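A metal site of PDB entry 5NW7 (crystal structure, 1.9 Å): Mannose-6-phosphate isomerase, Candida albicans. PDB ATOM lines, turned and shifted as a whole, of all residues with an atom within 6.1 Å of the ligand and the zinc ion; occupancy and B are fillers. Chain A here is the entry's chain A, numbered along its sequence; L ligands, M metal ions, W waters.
The side-chain amino group of Lys 324 lies within salt-bridge range of an oxygen (O6) of the ligand (2.5 Å). The side-chain carboxylate (OE1) of Glu 308 is in hydrogen-bond range of an oxygen (O7) of the ligand (2.6 Å). An oxygen (O1) of the ligand lies within hydrogen-bond range of the side-chain carboxylate of Glu 62, 2.6 Å away. An oxygen (O4) of the ligand sits close to the backbone NH (N) of Ser 123 (3.1 Å). OG of Ser 123 is in hydrogen-bond range of O4 of the ligand (2.7 Å). The indole nitrogen (NE1) of Trp 32 sits at hydrogen-bond distance from an oxygen (O6) of the ligand, at 2.9 Å. The side-chain amino group of Lys 150 lies within hydrogen-bond range of an oxygen (O7) of the ligand (3.3 Å). O5 of the ligand lies within salt-bridge range of NE of Arg 318, at 2.9 Å. The side-chain amino group of Lys 114 is in hydrogen-bond range of an oxygen (O1) of the ligand.
Residues that only touch the ligand: Tyr 301 (3.2 Å), Leu 122 (3.4 Å), Tyr 30 (3.7 Å) and Val 316 (3.8 Å). Hydrophobic or aromatic side chains that line the ligand: Tyr 30, Trp 32, Leu 122, His 127, His 299, Tyr 301 and Val 316.
Within 4 Å of the zinc ion: Gln 125, His 127, Glu 152 and His 299.
The zinc ion is bound by N2 of the ligand, OE2 of Glu 152, NE2 of His 299, O8 of the ligand, NE2 of His 127 and OE1 of Gln 125.
The side-chain carboxylate of Glu 152 sits at hydrogen-bond distance from the side-chain hydroxyl of Tyr 301 (2.9 Å). The side-chain amide nitrogen (NE2) of Gln 125 sits at hydrogen-bond distance from the side-chain hydroxyl (OG) of Ser 123, 2.9 Å away. The backbone NH (N) of Lys 324 sits at hydrogen-bond distance from the side-chain hydroxyl (OG1) of Thr 322 (2.9 Å). O of Glu 308 sits at hydrogen-bond distance from N of Lys 114 (2.8 Å). The side-chain carboxylate of Glu 62 is in salt-bridge range of the side-chain amino group of Lys 114 (2.6 Å). OE1 of Glu 62 is in hydrogen-bond range of NE1 of Trp 64. The side-chain amino group (NZ) of Lys 150 sits at hydrogen-bond distance from the side-chain sulfur (SD) of Met 310. The backbone NH (N) of Leu 122 is in hydrogen-bond range of the backbone carbonyl oxygen (O) of Tyr 301 (2.8 Å).
Water W4 lies within hydrogen-bond range of O4 of the ligand and OG1 of Thr 322. Water W5 lies within hydrogen-bond range of OH of Tyr 30 (2.6 Å), OD1 of Asp 314 (2.8 Å) and O1 of the ligand (2.8 Å). Water W3 lies within hydrogen-bond range of the side-chain amino group of Lys 324 (2.7 Å), the guanidinium group of Arg 318 (2.7 Å) and an oxygen (O5) of the ligand (2.9 Å). Water W2 lies within hydrogen-bond range of OD1 of Asp 314 (2.8 Å), O2 of the ligand (3.0 Å) and NZ of Lys 150 (3.1 Å). Water W1 lies within hydrogen-bond range of NE2 of Gln 125 (3.1 Å) and N of Tyr 301 (3.2 Å).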
ATOM      1  N   TYR A  30     -18.445 -10.354 -31.979  1.00  0.00           N
ATOM      2  CA  TYR A  30     -19.519  -9.671 -32.649  1.00  0.00           C
ATOM      3  C   TYR A  30     -19.404  -8.145 -32.365  1.00  0.00           C
ATOM      4  O   TYR A  30     -18.940  -7.726 -31.308  1.00  0.00           O
ATOM      5  CB  TYR A  30     -20.883 -10.175 -32.158  1.00  0.00           C
ATOM      6  CG  TYR A  30     -21.168 -11.669 -32.333  1.00  0.00           C
ATOM      7  CD1 TYR A  30     -20.587 -12.422 -33.382  1.00  0.00           C
ATOM      8  CD2 TYR A  30     -22.103 -12.310 -31.462  1.00  0.00           C
ATOM      9  CE1 TYR A  30     -20.894 -13.782 -33.540  1.00  0.00           C
ATOM     10  CE2 TYR A  30     -22.416 -13.665 -31.615  1.00  0.00           C
ATOM     11  CZ  TYR A  30     -21.822 -14.392 -32.639  1.00  0.00           C
ATOM     12  OH  TYR A  30     -22.189 -15.698 -32.794  1.00  0.00           O
ATOM     13  N   TRP A  32     -21.281  -5.744 -31.463  1.00  0.00           N
ATOM     14  CA  TRP A  32     -21.876  -5.151 -30.279  1.00  0.00           C
ATOM     15  C   TRP A  32     -21.113  -5.360 -28.974  1.00  0.00           C
ATOM     16  O   TRP A  32     -21.474  -4.804 -27.933  1.00  0.00           O
ATOM     17  CB  TRP A  32     -23.322  -5.591 -30.149  1.00  0.00           C
ATOM     18  CG  TRP A  32     -23.513  -7.071 -30.199  1.00  0.00           C
ATOM     19  CD1 TRP A  32     -24.032  -7.793 -31.233  1.00  0.00           C
ATOM     20  CD2 TRP A  32     -23.340  -7.949 -29.131  1.00  0.00           C
ATOM     21  NE1 TRP A  32     -24.158  -9.110 -30.872  1.00  0.00           N
ATOM     22  CE2 TRP A  32     -23.723  -9.239 -29.576  1.00  0.00           C
ATOM     23  CE3 TRP A  32     -22.840  -7.817 -27.801  1.00  0.00           C
ATOM     24  CZ2 TRP A  32     -23.679 -10.377 -28.740  1.00  0.00           C
ATOM     25  CZ3 TRP A  32     -22.762  -8.926 -26.995  1.00  0.00           C
ATOM     26  CH2 TRP A  32     -23.198 -10.222 -27.476  1.00  0.00           C
ATOM     27  N   GLU A  62     -19.051 -12.547 -26.770  1.00  0.00           N
ATOM     28  CA  GLU A  62     -19.584 -13.777 -26.145  1.00  0.00           C
ATOM     29  C   GLU A  62     -18.473 -14.760 -25.831  1.00  0.00           C
ATOM     30  O   GLU A  62     -17.590 -14.948 -26.668  1.00  0.00           O
ATOM     31  CB  GLU A  62     -20.584 -14.457 -27.080  1.00  0.00           C
ATOM     32  CG  GLU A  62     -21.699 -13.557 -27.603  1.00  0.00           C
ATOM     33  CD  GLU A  62     -22.866 -14.343 -28.151  1.00  0.00           C
ATOM     34  OE1 GLU A  62     -22.705 -15.541 -28.533  1.00  0.00           O
ATOM     35  OE2 GLU A  62     -23.969 -13.766 -28.283  1.00  0.00           O
ATOM     36  N   TRP A  64     -18.219 -18.753 -25.173  1.00  0.00           N
ATOM     37  CA  TRP A  64     -19.061 -19.965 -25.331  1.00  0.00           C
ATOM     38  C   TRP A  64     -18.487 -21.122 -24.548  1.00  0.00           C
ATOM     39  O   TRP A  64     -17.329 -21.437 -24.708  1.00  0.00           O
ATOM     40  CB  TRP A  64     -19.174 -20.391 -26.817  1.00  0.00           C
ATOM     41  CG  TRP A  64     -20.043 -19.528 -27.669  1.00  0.00           C
ATOM     42  CD1 TRP A  64     -20.181 -18.164 -27.604  1.00  0.00           C
ATOM     43  CD2 TRP A  64     -20.840 -19.951 -28.761  1.00  0.00           C
ATOM     44  NE1 TRP A  64     -21.037 -17.725 -28.579  1.00  0.00           N
ATOM     45  CE2 TRP A  64     -21.437 -18.810 -29.316  1.00  0.00           C
ATOM     46  CE3 TRP A  64     -21.123 -21.220 -29.320  1.00  0.00           C
ATOM     47  CZ2 TRP A  64     -22.283 -18.876 -30.402  1.00  0.00           C
ATOM     48  CZ3 TRP A  64     -21.969 -21.308 -30.383  1.00  0.00           C
ATOM     49  CH2 TRP A  64     -22.538 -20.136 -30.940  1.00  0.00           C
ATOM     50  N   LYS A 114     -23.041 -19.229 -21.601  1.00  0.00           N
ATOM     51  CA  LYS A 114     -22.254 -18.071 -22.142  1.00  0.00           C
ATOM     52  C   LYS A 114     -22.025 -16.967 -21.121  1.00  0.00           C
ATOM     53  O   LYS A 114     -22.855 -16.799 -20.203  1.00  0.00           O
ATOM     54  CB  LYS A 114     -23.014 -17.455 -23.327  1.00  0.00           C
ATOM     55  CG  LYS A 114     -23.151 -18.291 -24.586  1.00  0.00           C
ATOM     56  CD  LYS A 114     -23.746 -17.489 -25.730  1.00  0.00           C
ATOM     57  CE  LYS A 114     -24.076 -18.379 -26.927  1.00  0.00           C
ATOM     58  NZ  LYS A 114     -24.452 -17.469 -28.035  1.00  0.00           N
ATOM     59  N   LEU A 116     -21.931 -12.888 -21.758  1.00  0.00           N
ATOM     60  CA  LEU A 116     -22.040 -11.802 -22.703  1.00  0.00           C
ATOM     61  C   LEU A 116     -21.535 -10.507 -22.110  1.00  0.00           C
ATOM     62  O   LEU A 116     -21.810 -10.232 -20.929  1.00  0.00           O
ATOM     63  CB  LEU A 116     -23.477 -11.573 -23.181  1.00  0.00           C
ATOM     64  CG  LEU A 116     -23.938 -12.392 -24.415  1.00  0.00           C
ATOM     65  CD1 LEU A 116     -23.922 -13.872 -24.199  1.00  0.00           C
ATOM     66  CD2 LEU A 116     -25.329 -12.035 -24.925  1.00  0.00           C
ATOM     67  N   LEU A 122     -28.133  -5.620 -29.017  1.00  0.00           N
ATOM     68  CA  LEU A 122     -28.157  -6.749 -29.969  1.00  0.00           C
ATOM     69  C   LEU A 122     -29.268  -6.574 -30.945  1.00  0.00           C
ATOM     70  O   LEU A 122     -30.080  -5.673 -30.805  1.00  0.00           O
ATOM     71  CB  LEU A 122     -28.235  -8.166 -29.320  1.00  0.00           C
ATOM     72  CG  LEU A 122     -27.490  -8.539 -28.026  1.00  0.00           C
ATOM     73  CD1 LEU A 122     -27.332 -10.009 -27.774  1.00  0.00           C
ATOM     74  CD2 LEU A 122     -26.204  -7.765 -27.680  1.00  0.00           C
ATOM     75  N   SER A 123     -29.296  -7.463 -31.954  1.00  0.00           N
ATOM     76  CA  SER A 123     -30.406  -7.523 -32.882  1.00  0.00           C
ATOM     77  C   SER A 123     -31.730  -7.726 -32.155  1.00  0.00           C
ATOM     78  O   SER A 123     -31.781  -8.425 -31.175  1.00  0.00           O
ATOM     79  CB  SER A 123     -30.212  -8.617 -33.941  1.00  0.00           C
ATOM     80  OG  SER A 123     -30.349  -9.961 -33.361  1.00  0.00           O
ATOM     81  N   ILE A 124     -32.750  -7.065 -32.685  1.00  0.00           N
ATOM     82  CA  ILE A 124     -34.150  -7.434 -32.488  1.00  0.00           C
ATOM     83  C   ILE A 124     -34.241  -8.863 -33.012  1.00  0.00           C
ATOM     84  O   ILE A 124     -34.043  -9.115 -34.228  1.00  0.00           O
ATOM     85  CB  ILE A 124     -35.131  -6.498 -33.286  1.00  0.00           C
ATOM     86  CG1 ILE A 124     -34.927  -5.003 -32.927  1.00  0.00           C
ATOM     87  CG2 ILE A 124     -36.562  -6.940 -33.028  1.00  0.00           C
ATOM     88  CD1 ILE A 124     -35.093  -4.676 -31.479  1.00  0.00           C
ATOM     89  N   GLN A 125     -34.506  -9.789 -32.121  1.00  0.00           N
ATOM     90  CA  GLN A 125     -34.365 -11.191 -32.417  1.00  0.00           C
ATOM     91  C   GLN A 125     -35.397 -12.076 -31.741  1.00  0.00           C
ATOM     92  O   GLN A 125     -36.008 -11.743 -30.702  1.00  0.00           O
ATOM     93  CB  GLN A 125     -32.971 -11.658 -32.099  1.00  0.00           C
ATOM     94  CG  GLN A 125     -32.704 -11.809 -30.618  1.00  0.00           C
ATOM     95  CD  GLN A 125     -31.248 -12.061 -30.258  1.00  0.00           C
ATOM     96  OE1 GLN A 125     -30.914 -13.054 -29.494  1.00  0.00           O
ATOM     97  NE2 GLN A 125     -30.410 -11.107 -30.674  1.00  0.00           N
ATOM     98  N   HIS A 127     -35.863 -16.636 -31.315  1.00  0.00           N
ATOM     99  CA  HIS A 127     -35.318 -17.960 -31.577  1.00  0.00           C
ATOM    100  C   HIS A 127     -36.493 -18.936 -31.840  1.00  0.00           C
ATOM    101  O   HIS A 127     -37.560 -18.823 -31.200  1.00  0.00           O
ATOM    102  CB  HIS A 127     -34.496 -18.423 -30.412  1.00  0.00           C
ATOM    103  CG  HIS A 127     -33.429 -17.432 -30.010  1.00  0.00           C
ATOM    104  ND1 HIS A 127     -32.381 -17.095 -30.837  1.00  0.00           N
ATOM    105  CD2 HIS A 127     -33.292 -16.686 -28.892  1.00  0.00           C
ATOM    106  CE1 HIS A 127     -31.620 -16.189 -30.224  1.00  0.00           C
ATOM    107  NE2 HIS A 127     -32.178 -15.891 -29.052  1.00  0.00           N
ATOM    108  N   LYS A 150     -34.450 -22.637 -29.110  1.00  0.00           N
ATOM    109  CA  LYS A 150     -33.568 -21.933 -28.149  1.00  0.00           C
ATOM    110  C   LYS A 150     -34.294 -21.012 -27.146  1.00  0.00           C
ATOM    111  O   LYS A 150     -34.114 -19.813 -27.122  1.00  0.00           O
ATOM    112  CB  LYS A 150     -32.460 -21.209 -28.863  1.00  0.00           C
ATOM    113  CG  LYS A 150     -31.263 -20.892 -27.984  1.00  0.00           C
ATOM    114  CD  LYS A 150     -30.223 -20.009 -28.687  1.00  0.00           C
ATOM    115  CE  LYS A 150     -30.277 -18.599 -28.156  1.00  0.00           C
ATOM    116  NZ  LYS A 150     -28.992 -17.921 -28.588  1.00  0.00           N
ATOM    117  N   GLU A 152     -34.031 -19.420 -23.603  1.00  0.00           N
ATOM    118  CA  GLU A 152     -32.816 -18.969 -22.901  1.00  0.00           C
ATOM    119  C   GLU A 152     -33.099 -18.263 -21.583  1.00  0.00           C
ATOM    120  O   GLU A 152     -34.251 -17.886 -21.264  1.00  0.00           O
ATOM    121  CB  GLU A 152     -32.038 -18.062 -23.827  1.00  0.00           C
ATOM    122  CG  GLU A 152     -32.730 -16.809 -24.258  1.00  0.00           C
ATOM    123  CD  GLU A 152     -31.844 -15.854 -25.077  1.00  0.00           C
ATOM    124  OE1 GLU A 152     -31.046 -15.103 -24.462  1.00  0.00           O
ATOM    125  OE2 GLU A 152     -31.998 -15.757 -26.321  1.00  0.00           O
ATOM    126  N   HIS A 299     -36.952 -10.182 -28.479  1.00  0.00           N
ATOM    127  CA  HIS A 299     -36.059  -9.581 -27.487  1.00  0.00           C
ATOM    128  C   HIS A 299     -34.816  -8.946 -28.104  1.00  0.00           C
ATOM    129  O   HIS A 299     -34.458  -9.180 -29.272  1.00  0.00           O
ATOM    130  CB  HIS A 299     -35.590 -10.579 -26.403  1.00  0.00           C
ATOM    131  CG  HIS A 299     -34.823 -11.761 -26.899  1.00  0.00           C
ATOM    132  ND1 HIS A 299     -35.438 -12.812 -27.562  1.00  0.00           N
ATOM    133  CD2 HIS A 299     -33.513 -12.107 -26.784  1.00  0.00           C
ATOM    134  CE1 HIS A 299     -34.530 -13.746 -27.837  1.00  0.00           C
ATOM    135  NE2 HIS A 299     -33.347 -13.326 -27.412  1.00  0.00           N
ATOM    136  N   TYR A 301     -31.087  -7.521 -26.112  1.00  0.00           N
ATOM    137  CA  TYR A 301     -30.332  -7.093 -24.906  1.00  0.00           C
ATOM    138  C   TYR A 301     -29.628  -5.799 -25.227  1.00  0.00           C
ATOM    139  O   TYR A 301     -29.097  -5.649 -26.354  1.00  0.00           O
ATOM    140  CB  TYR A 301     -29.369  -8.207 -24.434  1.00  0.00           C
ATOM    141  CG  TYR A 301     -30.090  -9.530 -23.992  1.00  0.00           C
ATOM    142  CD1 TYR A 301     -31.496  -9.545 -23.792  1.00  0.00           C
ATOM    143  CD2 TYR A 301     -29.422 -10.750 -23.825  1.00  0.00           C
ATOM    144  CE1 TYR A 301     -32.181 -10.715 -23.437  1.00  0.00           C
ATOM    145  CE2 TYR A 301     -30.124 -11.927 -23.481  1.00  0.00           C
ATOM    146  CZ  TYR A 301     -31.499 -11.888 -23.268  1.00  0.00           C
ATOM    147  OH  TYR A 301     -32.282 -12.988 -22.912  1.00  0.00           O
ATOM    148  N   GLU A 308     -25.552 -16.101 -19.553  1.00  0.00           N
ATOM    149  CA  GLU A 308     -26.670 -16.590 -20.309  1.00  0.00           C
ATOM    150  C   GLU A 308     -26.594 -18.107 -20.353  1.00  0.00           C
ATOM    151  O   GLU A 308     -25.496 -18.725 -20.404  1.00  0.00           O
ATOM    152  CB  GLU A 308     -26.615 -15.939 -21.672  1.00  0.00           C
ATOM    153  CG  GLU A 308     -27.865 -15.767 -22.487  1.00  0.00           C
ATOM    154  CD  GLU A 308     -27.527 -15.110 -23.836  1.00  0.00           C
ATOM    155  OE1 GLU A 308     -26.674 -15.631 -24.591  1.00  0.00           O
ATOM    156  OE2 GLU A 308     -28.048 -14.017 -24.127  1.00  0.00           O
ATOM    157  N   MET A 310     -28.800 -21.447 -22.397  1.00  0.00           N
ATOM    158  CA  MET A 310     -29.820 -21.696 -23.373  1.00  0.00           C
ATOM    159  C   MET A 310     -29.813 -23.152 -23.760  1.00  0.00           C
ATOM    160  O   MET A 310     -28.820 -23.832 -23.513  1.00  0.00           O
ATOM    161  CB  MET A 310     -29.533 -20.849 -24.613  1.00  0.00           C
ATOM    162  CG  MET A 310     -28.234 -21.119 -25.287  1.00  0.00           C
ATOM    163  SD  MET A 310     -27.343 -19.618 -25.803  1.00  0.00           S
ATOM    164  CE  MET A 310     -27.063 -18.868 -24.203  1.00  0.00           C
ATOM    165  N   ASP A 314     -27.699 -22.253 -32.135  1.00  0.00           N
ATOM    166  CA  ASP A 314     -27.385 -20.916 -32.529  1.00  0.00           C
ATOM    167  C   ASP A 314     -28.386 -20.446 -33.623  1.00  0.00           C
ATOM    168  O   ASP A 314     -28.041 -19.696 -34.514  1.00  0.00           O
ATOM    169  CB  ASP A 314     -25.934 -20.812 -33.028  1.00  0.00           C
ATOM    170  CG  ASP A 314     -25.420 -19.354 -32.982  1.00  0.00           C
ATOM    171  OD1 ASP A 314     -25.890 -18.586 -32.140  1.00  0.00           O
ATOM    172  OD2 ASP A 314     -24.544 -19.020 -33.795  1.00  0.00           O
ATOM    173  N   VAL A 316     -31.244 -18.084 -34.808  1.00  0.00           N
ATOM    174  CA  VAL A 316     -31.791 -16.791 -34.480  1.00  0.00           C
ATOM    175  C   VAL A 316     -32.350 -16.107 -35.697  1.00  0.00           C
ATOM    176  O   VAL A 316     -31.760 -16.099 -36.736  1.00  0.00           O
ATOM    177  CB  VAL A 316     -30.734 -15.894 -33.731  1.00  0.00           C
ATOM    178  CG1 VAL A 316     -29.502 -15.663 -34.572  1.00  0.00           C
ATOM    179  CG2 VAL A 316     -31.346 -14.568 -33.290  1.00  0.00           C
ATOM    180  N   ARG A 318     -33.426 -12.484 -36.980  1.00  0.00           N
ATOM    181  CA  ARG A 318     -33.123 -11.098 -36.597  1.00  0.00           C
ATOM    182  C   ARG A 318     -33.968 -10.190 -37.490  1.00  0.00           C
ATOM    183  O   ARG A 318     -34.214 -10.532 -38.626  1.00  0.00           O
ATOM    184  CB  ARG A 318     -31.667 -10.777 -36.865  1.00  0.00           C
ATOM    185  CG  ARG A 318     -30.712 -11.778 -36.247  1.00  0.00           C
ATOM    186  CD  ARG A 318     -29.280 -11.320 -36.447  1.00  0.00           C
ATOM    187  NE  ARG A 318     -28.341 -12.357 -36.102  1.00  0.00           N
ATOM    188  CZ  ARG A 318     -27.971 -13.375 -36.862  1.00  0.00           C
ATOM    189  NH1 ARG A 318     -28.453 -13.586 -38.088  1.00  0.00           N
ATOM    190  NH2 ARG A 318     -27.078 -14.237 -36.369  1.00  0.00           N
ATOM    191  N   PHE A 321     -31.617  -3.531 -35.696  1.00  0.00           N
ATOM    192  CA  PHE A 321     -30.400  -3.187 -34.952  1.00  0.00           C
ATOM    193  C   PHE A 321     -29.245  -4.181 -35.218  1.00  0.00           C
ATOM    194  O   PHE A 321     -28.592  -4.635 -34.288  1.00  0.00           O
ATOM    195  CB  PHE A 321     -30.605  -3.165 -33.427  1.00  0.00           C
ATOM    196  CG  PHE A 321     -31.509  -2.116 -32.886  1.00  0.00           C
ATOM    197  CD1 PHE A 321     -31.391  -0.783 -33.272  1.00  0.00           C
ATOM    198  CD2 PHE A 321     -32.322  -2.418 -31.817  1.00  0.00           C
ATOM    199  CE1 PHE A 321     -32.119   0.236 -32.634  1.00  0.00           C
ATOM    200  CE2 PHE A 321     -33.120  -1.429 -31.224  1.00  0.00           C
ATOM    201  CZ  PHE A 321     -33.007  -0.087 -31.626  1.00  0.00           C
ATOM    202  N   THR A 322     -28.955  -4.476 -36.452  1.00  0.00           N
ATOM    203  CA  THR A 322     -27.835  -5.387 -36.754  1.00  0.00           C
ATOM    204  C   THR A 322     -27.387  -5.271 -38.230  1.00  0.00           C
ATOM    205  O   THR A 322     -28.199  -5.135 -39.091  1.00  0.00           O
ATOM    206  CB  THR A 322     -28.216  -6.903 -36.463  1.00  0.00           C
ATOM    207  OG1 THR A 322     -27.112  -7.777 -36.712  1.00  0.00           O
ATOM    208  CG2 THR A 322     -29.366  -7.375 -37.381  1.00  0.00           C
ATOM    209  N   LYS A 324     -26.032  -8.059 -39.372  1.00  0.00           N
ATOM    210  CA  LYS A 324     -26.077  -9.497 -39.708  1.00  0.00           C
ATOM    211  C   LYS A 324     -27.340  -9.789 -40.503  1.00  0.00           C
ATOM    212  O   LYS A 324     -28.159  -8.872 -40.753  1.00  0.00           O
ATOM    213  CB  LYS A 324     -26.024 -10.380 -38.437  1.00  0.00           C
ATOM    214  CG  LYS A 324     -24.807 -10.160 -37.526  1.00  0.00           C
ATOM    215  CD  LYS A 324     -25.037 -10.893 -36.196  1.00  0.00           C
ATOM    216  CE  LYS A 324     -23.748 -11.201 -35.467  1.00  0.00           C
ATOM    217  NZ  LYS A 324     -23.933 -12.100 -34.315  1.00  0.00           N
HETATM  218  O1  LIG L   1     -25.668 -15.231 -29.542  1.00  0.00           O
HETATM  219  C1  LIG L   1     -27.581 -13.849 -30.142  1.00  0.00           C
HETATM  220  C2  LIG L   1     -26.593 -12.653 -30.172  1.00  0.00           C
HETATM  221  O2  LIG L   1     -27.776 -14.379 -31.461  1.00  0.00           O
HETATM  222  N1  LIG L   1     -29.105 -13.488 -26.774  1.00  0.00           N
HETATM  223  O3  LIG L   1     -27.211 -11.507 -30.827  1.00  0.00           O
HETATM  224  O4  LIG L   1     -27.716  -9.958 -32.775  1.00  0.00           O
HETATM  225  O5  LIG L   1     -27.442 -12.392 -33.293  1.00  0.00           O
HETATM  226  O6  LIG L   1     -25.386 -11.056 -32.564  1.00  0.00           O
HETATM  227  P1  LIG L   1     -26.946 -11.223 -32.411  1.00  0.00           P
HETATM  228  C3  LIG L   1     -27.069 -14.952 -29.282  1.00  0.00           C
HETATM  229  C4  LIG L   1     -27.294 -14.690 -27.796  1.00  0.00           C
HETATM  230  O7  LIG L   1     -26.850 -15.880 -27.140  1.00  0.00           O
HETATM  231  C5  LIG L   1     -28.752 -14.485 -27.540  1.00  0.00           C
HETATM  232  O8  LIG L   1     -29.650 -15.151 -28.083  1.00  0.00           O
HETATM  233  N2  LIG L   1     -30.451 -13.287 -26.408  1.00  0.00           N
HETATM  234 ZN    ZN M   1     -31.552 -14.337 -27.702  1.00  0.00          ZN
HETATM  235  O   HOH W   1     -31.039 -10.214 -27.758  1.00  0.00           O
HETATM  236  O   HOH W   2     -28.352 -17.303 -31.539  1.00  0.00           O
HETATM  237  O   HOH W   3     -25.492 -14.298 -34.128  1.00  0.00           O
HETATM  238  O   HOH W   4     -26.303  -8.165 -33.829  1.00  0.00           O
HETATM  239  O   HOH W   5     -24.659 -16.122 -31.965  1.00  0.00           O
